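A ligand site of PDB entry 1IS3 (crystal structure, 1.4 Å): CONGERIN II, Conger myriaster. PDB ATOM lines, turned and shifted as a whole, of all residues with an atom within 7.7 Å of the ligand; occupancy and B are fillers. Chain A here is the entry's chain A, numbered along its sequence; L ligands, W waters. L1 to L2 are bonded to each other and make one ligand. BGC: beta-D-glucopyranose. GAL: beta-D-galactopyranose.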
ATOM      1  N   ARG A  29      11.035 -21.287 -14.020  1.00  0.00           N
ATOM      2  CA  ARG A  29      10.138 -20.399 -14.763  1.00  0.00           C
ATOM      3  C   ARG A  29       9.422 -21.182 -15.861  1.00  0.00           C
ATOM      4  O   ARG A  29       9.903 -22.233 -16.311  1.00  0.00           O
ATOM      5  CB  ARG A  29      10.934 -19.244 -15.399  1.00  0.00           C
ATOM      6  CG  ARG A  29      11.994 -19.784 -16.343  1.00  0.00           C
ATOM      7  CD  ARG A  29      13.103 -18.857 -16.768  1.00  0.00           C
ATOM      8  NE  ARG A  29      12.676 -17.907 -17.749  1.00  0.00           N
ATOM      9  CZ  ARG A  29      13.326 -17.638 -18.894  1.00  0.00           C
ATOM     10  NH1 ARG A  29      12.798 -16.713 -19.675  1.00  0.00           N
ATOM     11  NH2 ARG A  29      14.428 -18.233 -19.330  1.00  0.00           N
ATOM     12  N   SER A  31       6.723 -20.200 -19.515  1.00  0.00           N
ATOM     13  CA  SER A  31       6.028 -19.107 -20.197  1.00  0.00           C
ATOM     14  C   SER A  31       4.866 -19.575 -21.052  1.00  0.00           C
ATOM     15  O   SER A  31       4.897 -20.723 -21.504  1.00  0.00           O
ATOM     16  CB  SER A  31       7.006 -18.325 -21.074  1.00  0.00           C
ATOM     17  OG  SER A  31       7.677 -19.057 -22.086  1.00  0.00           O
ATOM     18  N   ASN A  33       3.124 -18.349 -24.642  1.00  0.00           N
ATOM     19  CA  ASN A  33       3.579 -17.535 -25.780  1.00  0.00           C
ATOM     20  C   ASN A  33       2.528 -17.537 -26.897  1.00  0.00           C
ATOM     21  O   ASN A  33       2.015 -18.619 -27.205  1.00  0.00           O
ATOM     22  CB  ASN A  33       4.883 -18.113 -26.345  1.00  0.00           C
ATOM     23  CG  ASN A  33       5.964 -18.146 -25.298  1.00  0.00           C
ATOM     24  OD1 ASN A  33       6.566 -17.126 -25.029  1.00  0.00           O
ATOM     25  ND2 ASN A  33       6.209 -19.258 -24.600  1.00  0.00           N
ATOM     26  N   HIS A  44       4.717 -12.765 -24.895  1.00  0.00           N
ATOM     27  CA  HIS A  44       5.436 -13.728 -24.092  1.00  0.00           C
ATOM     28  C   HIS A  44       5.082 -13.439 -22.620  1.00  0.00           C
ATOM     29  O   HIS A  44       5.320 -12.306 -22.205  1.00  0.00           O
ATOM     30  CB  HIS A  44       6.940 -13.566 -24.331  1.00  0.00           C
ATOM     31  CG  HIS A  44       7.875 -14.321 -23.363  1.00  0.00           C
ATOM     32  ND1 HIS A  44       8.164 -15.612 -23.327  1.00  0.00           N
ATOM     33  CD2 HIS A  44       8.697 -13.732 -22.394  1.00  0.00           C
ATOM     34  CE1 HIS A  44       9.097 -15.853 -22.422  1.00  0.00           C
ATOM     35  NE2 HIS A  44       9.408 -14.710 -21.861  1.00  0.00           N
ATOM     36  N   MET A  45       4.556 -14.357 -21.806  1.00  0.00           N
ATOM     37  CA  MET A  45       4.226 -14.095 -20.415  1.00  0.00           C
ATOM     38  C   MET A  45       5.059 -15.117 -19.637  1.00  0.00           C
ATOM     39  O   MET A  45       4.774 -16.335 -19.623  1.00  0.00           O
ATOM     40  CB  MET A  45       2.756 -14.331 -20.271  1.00  0.00           C
ATOM     41  CG  MET A  45       2.344 -14.161 -18.850  1.00  0.00           C
ATOM     42  SD  MET A  45       0.582 -14.578 -18.732  1.00  0.00           S
ATOM     43  CE  MET A  45       0.325 -13.590 -17.308  1.00  0.00           C
ATOM     44  N   ASP A  46       6.129 -14.673 -18.990  1.00  0.00           N
ATOM     45  CA  ASP A  46       7.022 -15.544 -18.289  1.00  0.00           C
ATOM     46  C   ASP A  46       6.714 -15.504 -16.796  1.00  0.00           C
ATOM     47  O   ASP A  46       6.484 -14.438 -16.215  1.00  0.00           O
ATOM     48  CB  ASP A  46       8.439 -15.098 -18.592  1.00  0.00           C
ATOM     49  CG  ASP A  46       9.495 -16.137 -18.288  1.00  0.00           C
ATOM     50  OD1 ASP A  46       9.218 -17.329 -18.342  1.00  0.00           O
ATOM     51  OD2 ASP A  46      10.622 -15.767 -17.996  1.00  0.00           O
ATOM     52  N   HIS A  47       6.665 -16.673 -16.171  1.00  0.00           N
ATOM     53  CA  HIS A  47       6.283 -16.828 -14.778  1.00  0.00           C
ATOM     54  C   HIS A  47       7.560 -17.229 -14.071  1.00  0.00           C
ATOM     55  O   HIS A  47       8.016 -18.367 -14.247  1.00  0.00           O
ATOM     56  CB  HIS A  47       5.216 -17.936 -14.592  1.00  0.00           C
ATOM     57  CG  HIS A  47       3.987 -17.770 -15.461  1.00  0.00           C
ATOM     58  ND1 HIS A  47       3.942 -17.878 -16.802  1.00  0.00           N
ATOM     59  CD2 HIS A  47       2.714 -17.581 -15.007  1.00  0.00           C
ATOM     60  CE1 HIS A  47       2.687 -17.766 -17.185  1.00  0.00           C
ATOM     61  NE2 HIS A  47       1.968 -17.596 -16.095  1.00  0.00           N
ATOM     62  N   ARG A  48       8.168 -16.307 -13.316  1.00  0.00           N
ATOM     63  CA  ARG A  48       9.497 -16.574 -12.756  1.00  0.00           C
ATOM     64  C   ARG A  48       9.443 -16.850 -11.269  1.00  0.00           C
ATOM     65  O   ARG A  48       9.135 -15.949 -10.471  1.00  0.00           O
ATOM     66  CB  ARG A  48      10.402 -15.384 -13.015  1.00  0.00           C
ATOM     67  CG  ARG A  48      10.709 -15.212 -14.510  1.00  0.00           C
ATOM     68  CD  ARG A  48      11.465 -13.918 -14.827  1.00  0.00           C
ATOM     69  NE  ARG A  48      11.656 -13.774 -16.284  1.00  0.00           N
ATOM     70  CZ  ARG A  48      12.473 -12.901 -16.887  1.00  0.00           C
ATOM     71  NH1 ARG A  48      12.572 -12.852 -18.226  1.00  0.00           N
ATOM     72  NH2 ARG A  48      13.166 -12.056 -16.144  1.00  0.00           N
ATOM     73  N   TYR A  51      14.681 -16.813 -11.193  1.00  0.00           N
ATOM     74  CA  TYR A  51      15.409 -16.643 -12.431  1.00  0.00           C
ATOM     75  C   TYR A  51      16.256 -15.411 -12.266  1.00  0.00           C
ATOM     76  O   TYR A  51      15.740 -14.294 -12.269  1.00  0.00           O
ATOM     77  CB  TYR A  51      14.421 -16.471 -13.627  1.00  0.00           C
ATOM     78  CG  TYR A  51      15.115 -16.205 -14.963  1.00  0.00           C
ATOM     79  CD1 TYR A  51      15.929 -17.177 -15.547  1.00  0.00           C
ATOM     80  CD2 TYR A  51      14.931 -14.982 -15.600  1.00  0.00           C
ATOM     81  CE1 TYR A  51      16.556 -16.934 -16.772  1.00  0.00           C
ATOM     82  CE2 TYR A  51      15.541 -14.728 -16.829  1.00  0.00           C
ATOM     83  CZ  TYR A  51      16.355 -15.717 -17.407  1.00  0.00           C
ATOM     84  OH  TYR A  51      16.937 -15.449 -18.634  1.00  0.00           O
ATOM     85  N   ALA A  53      17.844 -12.478 -10.623  1.00  0.00           N
ATOM     86  CA  ALA A  53      17.366 -11.769  -9.453  1.00  0.00           C
ATOM     87  C   ALA A  53      15.862 -11.784  -9.359  1.00  0.00           C
ATOM     88  O   ALA A  53      15.337 -11.203  -8.415  1.00  0.00           O
ATOM     89  CB  ALA A  53      17.761 -10.305  -9.471  1.00  0.00           C
ATOM     90  N   ASP A  54      15.126 -12.351 -10.312  1.00  0.00           N
ATOM     91  CA  ASP A  54      13.672 -12.371 -10.289  1.00  0.00           C
ATOM     92  C   ASP A  54      13.087 -13.537  -9.529  1.00  0.00           C
ATOM     93  O   ASP A  54      13.410 -14.707  -9.808  1.00  0.00           O
ATOM     94  CB  ASP A  54      13.159 -12.417 -11.722  1.00  0.00           C
ATOM     95  CG  ASP A  54      13.328 -11.085 -12.436  1.00  0.00           C
ATOM     96  OD1 ASP A  54      13.142 -10.059 -11.789  1.00  0.00           O
ATOM     97  OD2 ASP A  54      13.609 -11.061 -13.623  1.00  0.00           O
ATOM     98  N   VAL A  59       6.859 -11.488 -16.107  1.00  0.00           N
ATOM     99  CA  VAL A  59       7.549 -10.601 -17.028  1.00  0.00           C
ATOM    100  C   VAL A  59       6.875 -10.786 -18.394  1.00  0.00           C
ATOM    101  O   VAL A  59       6.747 -11.928 -18.887  1.00  0.00           O
ATOM    102  CB  VAL A  59       9.053 -10.967 -17.080  1.00  0.00           C
ATOM    103  CG1 VAL A  59       9.789 -10.111 -18.132  1.00  0.00           C
ATOM    104  CG2 VAL A  59       9.683 -10.715 -15.699  1.00  0.00           C
ATOM    105  N   LEU A  60       6.424  -9.694 -19.014  1.00  0.00           N
ATOM    106  CA  LEU A  60       5.779  -9.726 -20.318  1.00  0.00           C
ATOM    107  C   LEU A  60       6.612  -9.000 -21.371  1.00  0.00           C
ATOM    108  O   LEU A  60       7.211  -7.946 -21.091  1.00  0.00           O
ATOM    109  CB  LEU A  60       4.396  -9.083 -20.228  1.00  0.00           C
ATOM    110  CG  LEU A  60       3.458  -9.914 -19.350  1.00  0.00           C
ATOM    111  CD1 LEU A  60       3.490  -9.367 -17.929  1.00  0.00           C
ATOM    112  CD2 LEU A  60       2.073  -9.877 -19.933  1.00  0.00           C
ATOM    113  N   ASN A  61       6.683  -9.557 -22.580  1.00  0.00           N
ATOM    114  CA  ASN A  61       7.458  -8.936 -23.644  1.00  0.00           C
ATOM    115  C   ASN A  61       7.103  -9.486 -25.016  1.00  0.00           C
ATOM    116  O   ASN A  61       6.270 -10.404 -25.112  1.00  0.00           O
ATOM    117  CB  ASN A  61       8.967  -9.145 -23.361  1.00  0.00           C
ATOM    118  CG  ASN A  61       9.896  -8.059 -23.921  1.00  0.00           C
ATOM    119  OD1 ASN A  61       9.523  -7.249 -24.753  1.00  0.00           O
ATOM    120  ND2 ASN A  61      11.149  -8.029 -23.532  1.00  0.00           N
ATOM    121  N   SER A  62       7.613  -8.897 -26.094  1.00  0.00           N
ATOM    122  CA  SER A  62       7.449  -9.410 -27.439  1.00  0.00           C
ATOM    123  C   SER A  62       8.854  -9.686 -27.967  1.00  0.00           C
ATOM    124  O   SER A  62       9.855  -9.047 -27.563  1.00  0.00           O
ATOM    125  CB  SER A  62       6.715  -8.365 -28.254  1.00  0.00           C
ATOM    126  OG  SER A  62       7.453  -7.145 -28.241  1.00  0.00           O
ATOM    127  N   LEU A  63       8.905 -10.626 -28.896  1.00  0.00           N
ATOM    128  CA  LEU A  63      10.114 -11.080 -29.532  1.00  0.00           C
ATOM    129  C   LEU A  63       9.918 -10.897 -31.014  1.00  0.00           C
ATOM    130  O   LEU A  63       8.920 -11.402 -31.565  1.00  0.00           O
ATOM    131  CB  LEU A  63      10.356 -12.567 -29.240  1.00  0.00           C
ATOM    132  CG  LEU A  63      11.554 -13.236 -29.881  1.00  0.00           C
ATOM    133  CD1 LEU A  63      12.852 -12.652 -29.374  1.00  0.00           C
ATOM    134  CD2 LEU A  63      11.547 -14.697 -29.503  1.00  0.00           C
ATOM    135  N   TRP A  69      14.258  -9.369 -28.197  1.00  0.00           N
ATOM    136  CA  TRP A  69      13.301  -8.963 -27.193  1.00  0.00           C
ATOM    137  C   TRP A  69      13.152  -7.454 -27.134  1.00  0.00           C
ATOM    138  O   TRP A  69      14.149  -6.744 -27.296  1.00  0.00           O
ATOM    139  CB  TRP A  69      13.748  -9.537 -25.820  1.00  0.00           C
ATOM    140  CG  TRP A  69      13.581 -11.061 -25.735  1.00  0.00           C
ATOM    141  CD1 TRP A  69      14.659 -11.907 -25.807  1.00  0.00           C
ATOM    142  CD2 TRP A  69      12.384 -11.766 -25.659  1.00  0.00           C
ATOM    143  NE1 TRP A  69      14.173 -13.138 -25.768  1.00  0.00           N
ATOM    144  CE2 TRP A  69      12.829 -13.103 -25.681  1.00  0.00           C
ATOM    145  CE3 TRP A  69      11.006 -11.476 -25.573  1.00  0.00           C
ATOM    146  CZ2 TRP A  69      11.875 -14.147 -25.626  1.00  0.00           C
ATOM    147  CZ3 TRP A  69      10.081 -12.517 -25.526  1.00  0.00           C
ATOM    148  CH2 TRP A  69      10.521 -13.840 -25.546  1.00  0.00           C
ATOM    149  N   GLN A  70      11.934  -6.967 -26.940  1.00  0.00           N
ATOM    150  CA  GLN A  70      11.641  -5.550 -26.905  1.00  0.00           C
ATOM    151  C   GLN A  70      11.599  -5.064 -25.450  1.00  0.00           C
ATOM    152  O   GLN A  70      12.367  -5.592 -24.632  1.00  0.00           O
ATOM    153  CB  GLN A  70      10.318  -5.340 -27.663  1.00  0.00           C
ATOM    154  CG  GLN A  70      10.520  -5.780 -29.139  1.00  0.00           C
ATOM    155  CD  GLN A  70      11.740  -5.146 -29.846  1.00  0.00           C
ATOM    156  OE1 GLN A  70      11.803  -3.928 -30.018  1.00  0.00           O
ATOM    157  NE2 GLN A  70      12.742  -5.917 -30.270  1.00  0.00           N
ATOM    158  N   GLN A  71      10.779  -4.086 -25.092  1.00  0.00           N
ATOM    159  CA  GLN A  71      10.779  -3.540 -23.745  1.00  0.00           C
ATOM    160  C   GLN A  71       9.930  -4.444 -22.827  1.00  0.00           C
ATOM    161  O   GLN A  71       8.747  -4.687 -23.087  1.00  0.00           O
ATOM    162  CB  GLN A  71      10.231  -2.132 -23.866  1.00  0.00           C
ATOM    163  CG  GLN A  71      10.145  -1.339 -22.585  1.00  0.00           C
ATOM    164  CD  GLN A  71       8.750  -0.780 -22.215  1.00  0.00           C
ATOM    165  OE1 GLN A  71       8.272   0.265 -22.701  1.00  0.00           O
ATOM    166  NE2 GLN A  71       8.033  -1.430 -21.275  1.00  0.00           N
ATOM    167  N   GLU A  72      10.511  -4.955 -21.741  1.00  0.00           N
ATOM    168  CA  GLU A  72       9.796  -5.758 -20.729  1.00  0.00           C
ATOM    169  C   GLU A  72       8.801  -4.965 -19.903  1.00  0.00           C
ATOM    170  O   GLU A  72       9.057  -3.795 -19.559  1.00  0.00           O
ATOM    171  CB  GLU A  72      10.666  -6.354 -19.649  1.00  0.00           C
ATOM    172  CG  GLU A  72      11.805  -7.122 -20.170  1.00  0.00           C
ATOM    173  CD  GLU A  72      12.592  -7.820 -19.088  1.00  0.00           C
ATOM    174  OE1 GLU A  72      12.697  -7.353 -17.945  1.00  0.00           O
ATOM    175  OE2 GLU A  72      13.121  -8.853 -19.423  1.00  0.00           O
ATOM    176  N   GLU A  73       7.688  -5.582 -19.550  1.00  0.00           N
ATOM    177  CA  GLU A  73       6.734  -5.032 -18.607  1.00  0.00           C
ATOM    178  C   GLU A  73       6.694  -6.066 -17.513  1.00  0.00           C
ATOM    179  O   GLU A  73       6.848  -7.259 -17.778  1.00  0.00           O
ATOM    180  CB  GLU A  73       5.384  -4.878 -19.258  1.00  0.00           C
ATOM    181  CG  GLU A  73       5.547  -3.580 -20.094  1.00  0.00           C
ATOM    182  CD  GLU A  73       4.328  -2.952 -20.756  1.00  0.00           C
ATOM    183  OE1 GLU A  73       4.512  -2.215 -21.752  1.00  0.00           O
ATOM    184  OE2 GLU A  73       3.205  -3.183 -20.283  1.00  0.00           O
ATOM    185  N   ARG A  74       6.637  -5.635 -16.264  1.00  0.00           N
ATOM    186  CA  ARG A  74       6.625  -6.558 -15.124  1.00  0.00           C
ATOM    187  C   ARG A  74       5.415  -6.431 -14.225  1.00  0.00           C
ATOM    188  O   ARG A  74       4.840  -5.343 -14.115  1.00  0.00           O
ATOM    189  CB  ARG A  74       7.870  -6.349 -14.280  1.00  0.00           C
ATOM    190  CG  ARG A  74       9.091  -6.858 -15.025  1.00  0.00           C
ATOM    191  CD  ARG A  74      10.400  -6.178 -14.653  1.00  0.00           C
ATOM    192  NE  ARG A  74      11.529  -6.843 -15.304  1.00  0.00           N
ATOM    193  CZ  ARG A  74      12.082  -7.925 -14.724  1.00  0.00           C
ATOM    194  NH1 ARG A  74      11.618  -8.384 -13.560  1.00  0.00           N
ATOM    195  NH2 ARG A  74      13.108  -8.553 -15.305  1.00  0.00           N
HETATM  196  C2  BGC L   1      16.377  -9.011 -17.787  1.00  0.00           C
HETATM  197  C3  BGC L   1      15.783 -10.401 -18.018  1.00  0.00           C
HETATM  198  C4  BGC L   1      16.175 -10.894 -19.407  1.00  0.00           C
HETATM  199  C5  BGC L   1      17.709 -10.873 -19.556  1.00  0.00           C
HETATM  200  C6  BGC L   1      18.172 -11.230 -20.952  1.00  0.00           C
HETATM  201  C1  BGC L   1      17.898  -9.091 -17.969  1.00  0.00           C
HETATM  202  O1  BGC L   1      18.443  -7.830 -17.801  1.00  0.00           O
HETATM  203  O2  BGC L   1      16.063  -8.557 -16.480  1.00  0.00           O
HETATM  204  O3  BGC L   1      14.377 -10.354 -17.897  1.00  0.00           O
HETATM  205  O4  BGC L   1      15.711 -12.240 -19.591  1.00  0.00           O
HETATM  206  O5  BGC L   1      18.208  -9.536 -19.287  1.00  0.00           O
HETATM  207  O6  BGC L   1      17.585 -10.384 -21.924  1.00  0.00           O
HETATM  208  C1  GAL L   2      15.017 -12.515 -20.766  1.00  0.00           C
HETATM  209  C2  GAL L   2      14.898 -14.030 -20.914  1.00  0.00           C
HETATM  210  C3  GAL L   2      14.011 -14.386 -22.085  1.00  0.00           C
HETATM  211  C4  GAL L   2      12.661 -13.670 -21.974  1.00  0.00           C
HETATM  212  C5  GAL L   2      12.907 -12.169 -21.828  1.00  0.00           C
HETATM  213  C6  GAL L   2      11.631 -11.386 -21.678  1.00  0.00           C
HETATM  214  O2  GAL L   2      16.181 -14.583 -21.101  1.00  0.00           O
HETATM  215  O3  GAL L   2      13.806 -15.794 -22.128  1.00  0.00           O
HETATM  216  O4  GAL L   2      11.924 -14.147 -20.860  1.00  0.00           O
HETATM  217  O5  GAL L   2      13.715 -11.911 -20.662  1.00  0.00           O
HETATM  218  O6  GAL L   2      11.905  -9.999 -21.621  1.00  0.00           O
HETATM  219  O   HOH W   1      16.086 -10.802 -14.568  1.00  0.00           O
HETATM  220  O   HOH W   2      18.942 -14.417 -22.957  1.00  0.00           O
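Water W1 lies within hydrogen-bond range of OD2 of Asp 54 and O2 of BGC L1.
NH2 of Arg 74 lies within salt-bridge range of OE1 of Glu 72 (2.9 Å). NH2 of Arg 48 is in salt-bridge range of OD2 of Asp 54 (2.7 Å). ND1 of His 44 lies within hydrogen-bond range of OD1 of Asn 33. NH1 of Arg 29 lies within salt-bridge range of OD2 of Asp 46, at 2.9 Å. O of Gln 70 is in hydrogen-bond range of ND2 of Asn 61, 2.9 Å away. The backbone carbonyl oxygen (O) of Gln 71 sits close to the side-chain amide oxygen (OD1) of Asn 61, 3.2 Å away. The guanidinium group (NH1) of Arg 74 lies within salt-bridge range of the side-chain carboxylate (OD1) of Asp 54 (2.9 Å). N of Asp 46 sits at hydrogen-bond distance from O of Val 59, 2.8 Å away.
Merely in contact with the ligand: Asp 46 and Trp 69. Hydrophobic or aromatic side chains that line the ligand: His 44, Tyr 51 and Trp 69. The nearest printed residue that does not touch the ligand is Val 59 (4.1 Å).
The side-chain carboxylate (OE2) of Glu 72 sits at hydrogen-bond distance from an oxygen (O3) of BGC L1. The side-chain hydroxyl (OH) of Tyr 51 lies within hydrogen-bond range of an oxygen (O2) of GAL L2 (2.7 Å). The guanidinium group (NH2) of Arg 48 sits at hydrogen-bond distance from an oxygen (O3) of BGC L1. An oxygen (O4) of GAL L2 is in hydrogen-bond range of a ring nitrogen (NE2) of His 44, 2.8 Å away. NH1 of Arg 29 lies within hydrogen-bond range of O3 of GAL L2 (2.8 Å). The side-chain amide nitrogen (ND2) of Asn 61 is in hydrogen-bond range of an oxygen (O6) of GAL L2 (2.8 Å). The guanidinium group (NH2) of Arg 74 lies within hydrogen-bond range of an oxygen (O2) of BGC L1 (3.2 Å).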
